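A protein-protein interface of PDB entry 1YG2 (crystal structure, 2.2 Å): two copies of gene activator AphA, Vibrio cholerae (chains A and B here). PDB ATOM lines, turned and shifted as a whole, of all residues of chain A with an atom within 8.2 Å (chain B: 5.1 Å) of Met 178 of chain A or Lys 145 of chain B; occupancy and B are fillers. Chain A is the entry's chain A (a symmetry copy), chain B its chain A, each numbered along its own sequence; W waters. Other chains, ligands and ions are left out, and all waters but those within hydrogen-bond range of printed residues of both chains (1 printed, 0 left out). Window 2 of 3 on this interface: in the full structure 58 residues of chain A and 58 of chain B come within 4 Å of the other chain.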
ATOM      1  N   LEU A 100      19.830 -19.319  32.538  1.00  0.00           N
ATOM      2  CA  LEU A 100      20.163 -18.039  31.921  1.00  0.00           C
ATOM      3  C   LEU A 100      21.168 -18.251  30.796  1.00  0.00           C
ATOM      4  O   LEU A 100      20.990 -17.751  29.692  1.00  0.00           O
ATOM      5  CB  LEU A 100      20.768 -17.091  32.957  1.00  0.00           C
ATOM      6  CG  LEU A 100      20.457 -15.589  32.935  1.00  0.00           C
ATOM      7  CD1 LEU A 100      21.728 -14.864  33.311  1.00  0.00           C
ATOM      8  CD2 LEU A 100      19.950 -15.107  31.577  1.00  0.00           C
ATOM      9  N   MET A 101      22.226 -19.003  31.068  1.00  0.00           N
ATOM     10  CA  MET A 101      23.227 -19.233  30.039  1.00  0.00           C
ATOM     11  C   MET A 101      22.663 -19.917  28.803  1.00  0.00           C
ATOM     12  O   MET A 101      23.151 -19.710  27.700  1.00  0.00           O
ATOM     13  CB  MET A 101      24.392 -20.056  30.593  1.00  0.00           C
ATOM     14  CG  MET A 101      25.239 -19.317  31.627  1.00  0.00           C
ATOM     15  SD  MET A 101      25.740 -17.639  31.115  1.00  0.00           S
ATOM     16  CE  MET A 101      26.455 -17.949  29.523  1.00  0.00           C
ATOM     17  N   CYS A 103      20.007 -19.259  27.528  1.00  0.00           N
ATOM     18  CA  CYS A 103      19.202 -18.306  26.777  1.00  0.00           C
ATOM     19  C   CYS A 103      19.903 -17.861  25.502  1.00  0.00           C
ATOM     20  O   CYS A 103      19.282 -17.263  24.627  1.00  0.00           O
ATOM     21  CB  CYS A 103      18.850 -17.097  27.632  1.00  0.00           C
ATOM     22  SG  CYS A 103      17.531 -17.469  28.792  1.00  0.00           S
ATOM     23  N   SER A 104      21.195 -18.150  25.394  1.00  0.00           N
ATOM     24  CA  SER A 104      21.928 -17.779  24.192  1.00  0.00           C
ATOM     25  C   SER A 104      21.543 -18.719  23.048  1.00  0.00           C
ATOM     26  O   SER A 104      21.717 -18.386  21.878  1.00  0.00           O
ATOM     27  CB  SER A 104      23.436 -17.869  24.426  1.00  0.00           C
ATOM     28  OG  SER A 104      23.887 -19.210  24.309  1.00  0.00           O
ATOM     29  N   VAL A 105      21.019 -19.893  23.390  1.00  0.00           N
ATOM     30  CA  VAL A 105      20.631 -20.870  22.379  1.00  0.00           C
ATOM     31  C   VAL A 105      19.166 -21.290  22.460  1.00  0.00           C
ATOM     32  O   VAL A 105      18.697 -22.066  21.634  1.00  0.00           O
ATOM     33  CB  VAL A 105      21.503 -22.144  22.475  1.00  0.00           C
ATOM     34  CG1 VAL A 105      22.959 -21.795  22.226  1.00  0.00           C
ATOM     35  CG2 VAL A 105      21.345 -22.787  23.849  1.00  0.00           C
ATOM     36  N   GLN A 106      18.448 -20.784  23.455  1.00  0.00           N
ATOM     37  CA  GLN A 106      17.039 -21.126  23.629  1.00  0.00           C
ATOM     38  C   GLN A 106      16.165 -19.880  23.589  1.00  0.00           C
ATOM     39  O   GLN A 106      16.648 -18.765  23.789  1.00  0.00           O
ATOM     40  CB  GLN A 106      16.823 -21.825  24.975  1.00  0.00           C
ATOM     41  CG  GLN A 106      17.622 -23.101  25.186  1.00  0.00           C
ATOM     42  CD  GLN A 106      17.029 -24.298  24.469  1.00  0.00           C
ATOM     43  OE1 GLN A 106      16.979 -24.345  23.242  1.00  0.00           O
ATOM     44  NE2 GLN A 106      16.575 -25.275  25.237  1.00  0.00           N
ATOM     45  N   SER A 107      14.876 -20.071  23.329  1.00  0.00           N
ATOM     46  CA  SER A 107      13.941 -18.955  23.301  1.00  0.00           C
ATOM     47  C   SER A 107      13.870 -18.463  24.736  1.00  0.00           C
ATOM     48  O   SER A 107      13.439 -19.195  25.621  1.00  0.00           O
ATOM     49  CB  SER A 107      12.560 -19.427  22.838  1.00  0.00           C
ATOM     50  OG  SER A 107      12.062 -20.455  23.681  1.00  0.00           O
ATOM     51  N   ALA A 108      14.302 -17.228  24.965  1.00  0.00           N
ATOM     52  CA  ALA A 108      14.312 -16.656  26.307  1.00  0.00           C
ATOM     53  C   ALA A 108      12.922 -16.413  26.887  1.00  0.00           C
ATOM     54  O   ALA A 108      12.787 -16.043  28.054  1.00  0.00           O
ATOM     55  CB  ALA A 108      15.110 -15.356  26.302  1.00  0.00           C
ATOM     56  N   VAL A 171      18.644  -9.351  35.635  1.00  0.00           N
ATOM     57  CA  VAL A 171      18.549 -10.299  34.536  1.00  0.00           C
ATOM     58  C   VAL A 171      17.374  -9.918  33.649  1.00  0.00           C
ATOM     59  O   VAL A 171      17.505  -9.843  32.430  1.00  0.00           O
ATOM     60  CB  VAL A 171      18.327 -11.732  35.044  1.00  0.00           C
ATOM     61  CG1 VAL A 171      18.072 -12.663  33.863  1.00  0.00           C
ATOM     62  CG2 VAL A 171      19.540 -12.195  35.843  1.00  0.00           C
ATOM     63  N   LEU A 172      16.226  -9.678  34.276  1.00  0.00           N
ATOM     64  CA  LEU A 172      15.014  -9.306  33.553  1.00  0.00           C
ATOM     65  C   LEU A 172      15.259  -8.136  32.622  1.00  0.00           C
ATOM     66  O   LEU A 172      14.669  -8.062  31.545  1.00  0.00           O
ATOM     67  CB  LEU A 172      13.895  -8.974  34.541  1.00  0.00           C
ATOM     68  CG  LEU A 172      13.447 -10.196  35.344  1.00  0.00           C
ATOM     69  CD1 LEU A 172      12.407  -9.808  36.367  1.00  0.00           C
ATOM     70  CD2 LEU A 172      12.891 -11.241  34.394  1.00  0.00           C
ATOM     71  N   ALA A 173      16.143  -7.231  33.029  1.00  0.00           N
ATOM     72  CA  ALA A 173      16.470  -6.071  32.214  1.00  0.00           C
ATOM     73  C   ALA A 173      17.288  -6.483  30.998  1.00  0.00           C
ATOM     74  O   ALA A 173      16.958  -6.121  29.871  1.00  0.00           O
ATOM     75  CB  ALA A 173      17.240  -5.052  33.035  1.00  0.00           C
ATOM     76  N   GLU A 174      18.358  -7.237  31.230  1.00  0.00           N
ATOM     77  CA  GLU A 174      19.221  -7.688  30.146  1.00  0.00           C
ATOM     78  C   GLU A 174      18.453  -8.481  29.101  1.00  0.00           C
ATOM     79  O   GLU A 174      18.734  -8.390  27.906  1.00  0.00           O
ATOM     80  CB  GLU A 174      20.352  -8.560  30.691  1.00  0.00           C
ATOM     81  CG  GLU A 174      21.336  -7.837  31.590  1.00  0.00           C
ATOM     82  CD  GLU A 174      22.053  -6.702  30.889  1.00  0.00           C
ATOM     83  OE1 GLU A 174      22.555  -6.908  29.764  1.00  0.00           O
ATOM     84  OE2 GLU A 174      22.115  -5.601  31.472  1.00  0.00           O
ATOM     85  N   LEU A 175      17.488  -9.269  29.556  1.00  0.00           N
ATOM     86  CA  LEU A 175      16.697 -10.083  28.645  1.00  0.00           C
ATOM     87  C   LEU A 175      15.862  -9.238  27.677  1.00  0.00           C
ATOM     88  O   LEU A 175      15.223  -9.775  26.770  1.00  0.00           O
ATOM     89  CB  LEU A 175      15.809 -11.049  29.443  1.00  0.00           C
ATOM     90  CG  LEU A 175      16.573 -12.209  30.105  1.00  0.00           C
ATOM     91  CD1 LEU A 175      15.658 -13.012  31.009  1.00  0.00           C
ATOM     92  CD2 LEU A 175      17.166 -13.103  29.028  1.00  0.00           C
ATOM     93  N   ASN A 176      15.887  -7.918  27.861  1.00  0.00           N
ATOM     94  CA  ASN A 176      15.153  -7.003  26.986  1.00  0.00           C
ATOM     95  C   ASN A 176      16.119  -6.240  26.091  1.00  0.00           C
ATOM     96  O   ASN A 176      15.973  -6.225  24.872  1.00  0.00           O
ATOM     97  CB  ASN A 176      14.332  -5.994  27.795  1.00  0.00           C
ATOM     98  CG  ASN A 176      13.338  -6.656  28.721  1.00  0.00           C
ATOM     99  OD1 ASN A 176      12.846  -7.749  28.445  1.00  0.00           O
ATOM    100  ND2 ASN A 176      13.023  -5.987  29.824  1.00  0.00           N
ATOM    101  N   ALA A 177      17.105  -5.607  26.711  1.00  0.00           N
ATOM    102  CA  ALA A 177      18.098  -4.830  25.983  1.00  0.00           C
ATOM    103  C   ALA A 177      18.871  -5.652  24.955  1.00  0.00           C
ATOM    104  O   ALA A 177      19.561  -5.087  24.106  1.00  0.00           O
ATOM    105  CB  ALA A 177      19.069  -4.176  26.963  1.00  0.00           C
ATOM    106  N   MET A 178      18.765  -6.979  25.035  1.00  0.00           N
ATOM    107  CA  MET A 178      19.461  -7.856  24.094  1.00  0.00           C
ATOM    108  C   MET A 178      18.581  -8.117  22.877  1.00  0.00           C
ATOM    109  O   MET A 178      19.066  -8.180  21.746  1.00  0.00           O
ATOM    110  CB  MET A 178      19.815  -9.200  24.747  1.00  0.00           C
ATOM    111  CG  MET A 178      18.610 -10.120  24.980  1.00  0.00           C
ATOM    112  SD  MET A 178      19.023 -11.874  25.235  1.00  0.00           S
ATOM    113  CE  MET A 178      19.095 -12.456  23.515  1.00  0.00           C
ATOM    114  N   ALA A 179      17.283  -8.271  23.121  1.00  0.00           N
ATOM    115  CA  ALA A 179      16.324  -8.537  22.058  1.00  0.00           C
ATOM    116  C   ALA A 179      15.791  -7.231  21.483  1.00  0.00           C
ATOM    117  O   ALA A 179      16.076  -6.954  20.299  1.00  0.00           O
ATOM    118  CB  ALA A 179      15.179  -9.379  22.597  1.00  0.00           C
ATOM    119  OXT ALA A 179      15.105  -6.499  22.230  1.00  0.00           O
ATOM    120  N   LEU B 143      29.809  -5.145  25.980  1.00  0.00           N
ATOM    121  CA  LEU B 143      29.968  -6.594  25.977  1.00  0.00           C
ATOM    122  C   LEU B 143      29.020  -7.296  25.003  1.00  0.00           C
ATOM    123  O   LEU B 143      27.921  -6.808  24.740  1.00  0.00           O
ATOM    124  CB  LEU B 143      29.723  -7.127  27.388  1.00  0.00           C
ATOM    125  CG  LEU B 143      30.570  -6.527  28.508  1.00  0.00           C
ATOM    126  CD1 LEU B 143      30.078  -7.053  29.850  1.00  0.00           C
ATOM    127  CD2 LEU B 143      32.031  -6.872  28.289  1.00  0.00           C
ATOM    128  N   ASP B 144      29.448  -8.439  24.472  1.00  0.00           N
ATOM    129  CA  ASP B 144      28.612  -9.212  23.562  1.00  0.00           C
ATOM    130  C   ASP B 144      27.498  -9.843  24.393  1.00  0.00           C
ATOM    131  O   ASP B 144      27.526  -9.782  25.622  1.00  0.00           O
ATOM    132  CB  ASP B 144      29.407 -10.339  22.903  1.00  0.00           C
ATOM    133  CG  ASP B 144      30.742  -9.881  22.359  1.00  0.00           C
ATOM    134  OD1 ASP B 144      30.782  -8.846  21.653  1.00  0.00           O
ATOM    135  OD2 ASP B 144      31.748 -10.571  22.636  1.00  0.00           O
ATOM    136  N   LYS B 145      26.532 -10.460  23.719  1.00  0.00           N
ATOM    137  CA  LYS B 145      25.415 -11.107  24.398  1.00  0.00           C
ATOM    138  C   LYS B 145      25.917 -12.167  25.370  1.00  0.00           C
ATOM    139  O   LYS B 145      25.545 -12.178  26.540  1.00  0.00           O
ATOM    140  CB  LYS B 145      24.473 -11.751  23.379  1.00  0.00           C
ATOM    141  CG  LYS B 145      23.741 -10.750  22.503  1.00  0.00           C
ATOM    142  CD  LYS B 145      22.741 -11.430  21.570  1.00  0.00           C
ATOM    143  CE  LYS B 145      21.926 -10.407  20.777  1.00  0.00           C
ATOM    144  NZ  LYS B 145      20.854 -11.044  19.941  1.00  0.00           N
ATOM    145  N   GLN B 146      26.770 -13.049  24.869  1.00  0.00           N
ATOM    146  CA  GLN B 146      27.345 -14.121  25.667  1.00  0.00           C
ATOM    147  C   GLN B 146      28.044 -13.573  26.919  1.00  0.00           C
ATOM    148  O   GLN B 146      27.992 -14.188  27.984  1.00  0.00           O
ATOM    149  CB  GLN B 146      28.337 -14.910  24.806  1.00  0.00           C
ATOM    150  CG  GLN B 146      28.836 -16.200  25.414  1.00  0.00           C
ATOM    151  CD  GLN B 146      27.707 -17.141  25.787  1.00  0.00           C
ATOM    152  OE1 GLN B 146      26.589 -17.018  25.286  1.00  0.00           O
ATOM    153  NE2 GLN B 146      27.998 -18.095  26.661  1.00  0.00           N
ATOM    154  N   GLN B 147      28.683 -12.413  26.792  1.00  0.00           N
ATOM    155  CA  GLN B 147      29.388 -11.796  27.916  1.00  0.00           C
ATOM    156  C   GLN B 147      28.431 -11.188  28.926  1.00  0.00           C
ATOM    157  O   GLN B 147      28.686 -11.222  30.130  1.00  0.00           O
ATOM    158  CB  GLN B 147      30.346 -10.709  27.421  1.00  0.00           C
ATOM    159  CG  GLN B 147      31.463 -11.212  26.527  1.00  0.00           C
ATOM    160  CD  GLN B 147      32.331 -10.079  26.006  1.00  0.00           C
ATOM    161  OE1 GLN B 147      31.868  -9.225  25.249  1.00  0.00           O
ATOM    162  NE2 GLN B 147      33.594 -10.064  26.419  1.00  0.00           N
ATOM    163  N   ARG B 148      27.334 -10.618  28.441  1.00  0.00           N
ATOM    164  CA  ARG B 148      26.364 -10.027  29.353  1.00  0.00           C
ATOM    165  C   ARG B 148      25.755 -11.124  30.215  1.00  0.00           C
ATOM    166  O   ARG B 148      25.471 -10.912  31.389  1.00  0.00           O
ATOM    167  CB  ARG B 148      25.260  -9.294  28.594  1.00  0.00           C
ATOM    168  CG  ARG B 148      25.713  -8.024  27.905  1.00  0.00           C
ATOM    169  CD  ARG B 148      24.528  -7.093  27.677  1.00  0.00           C
ATOM    170  NE  ARG B 148      24.469  -6.593  26.307  1.00  0.00           N
ATOM    171  CZ  ARG B 148      24.017  -7.295  25.271  1.00  0.00           C
ATOM    172  NH1 ARG B 148      23.574  -8.536  25.441  1.00  0.00           N
ATOM    173  NH2 ARG B 148      24.010  -6.757  24.058  1.00  0.00           N
ATOM    174  N   LEU B 149      25.553 -12.293  29.619  1.00  0.00           N
ATOM    175  CA  LEU B 149      25.001 -13.432  30.338  1.00  0.00           C
ATOM    176  C   LEU B 149      25.997 -13.897  31.413  1.00  0.00           C
ATOM    177  O   LEU B 149      25.617 -14.092  32.571  1.00  0.00           O
ATOM    178  CB  LEU B 149      24.706 -14.576  29.364  1.00  0.00           C
ATOM    179  CG  LEU B 149      23.587 -14.336  28.342  1.00  0.00           C
ATOM    180  CD1 LEU B 149      23.373 -15.603  27.521  1.00  0.00           C
ATOM    181  CD2 LEU B 149      22.300 -13.944  29.060  1.00  0.00           C
HETATM  182  O   HOH W   1      26.300 -20.273  27.155  1.00  0.00           O
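SG of Cys 103 of chain A sits close to O of Leu 100 of chain A, 3.6 Å away.
The guanidinium group (NE) of Arg 148 of chain B is in salt-bridge range of the side-chain carboxylate (OE1) of Glu 174 of chain A, 3.96 Å away.
No position is printed for both chains.
Of the 8 pairs that touch across the chains among the printed residues, none has its exchanged pair printed and touching as well.
Leu 149 of chain B touches Leu 100 of chain A (CD2 to CD2, 3.6 Å).
Gln 146 of chain B touches Met 101 of chain A (NE2 to CE, 3.3 Å).
SD of Met 101 of chain A touches CB of Leu 149 of chain B, at 3.7 Å.
CB of Ser 104 of chain A touches OE1 of Gln 146 of chain B, 3.4 Å away.
Leu 149 of chain B touches Ser 104 of chain A.
Met 178 of chain A touches Lys 145 of chain B.
Met 178 of chain A touches Arg 148 of chain B.
Water W1 bridges NE2 of Gln 146 of chain B (2.8 Å) and O of Met 101 of chain A (3.2 Å).
Printed residues of chain B that touch a printed residue of chain A: Lys 145, Gln 146, Arg 148 and Leu 149.
Hydrophobic or aromatic side chains of chain A that line the printed part of chain B: Leu 100, Met 101 and Met 178.
Among the printed residues, 8 pairs touch across the chains.
Among the printed residues, Asp or Glu carboxylates within 4 Å of a Lys or Arg side-chain nitrogen of the other chain: Glu 174 of chain A with Arg 148 of chain B.
Met 178 of chain A touches just these residues of chain B: Lys 145 (3.8 Å) and Arg 148 (3.9 Å).
Lys 145 of chain B touches just one residue of chain A: Met 178.
Of the printed residues of chain B, Glu 174 of chain A touches Arg 148.
Of the printed residues of chain A, Leu 149 of chain B touches Leu 100 (3.6 Å), Met 101 (3.7 Å) and Ser 104 (3.8 Å).
Val 171 of chain A touches none of the printed residues of chain B.
Cys 103 of chain A touches none of the printed residues of chain B.
The nearest residue of chain A that does not touch Lys 145 of chain B is Ala 179 of chain A (5.5 Å).
The nearest printed residue of chain B that does not touch Ser 104 of chain A is Lys 145 of chain B (6.3 Å).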
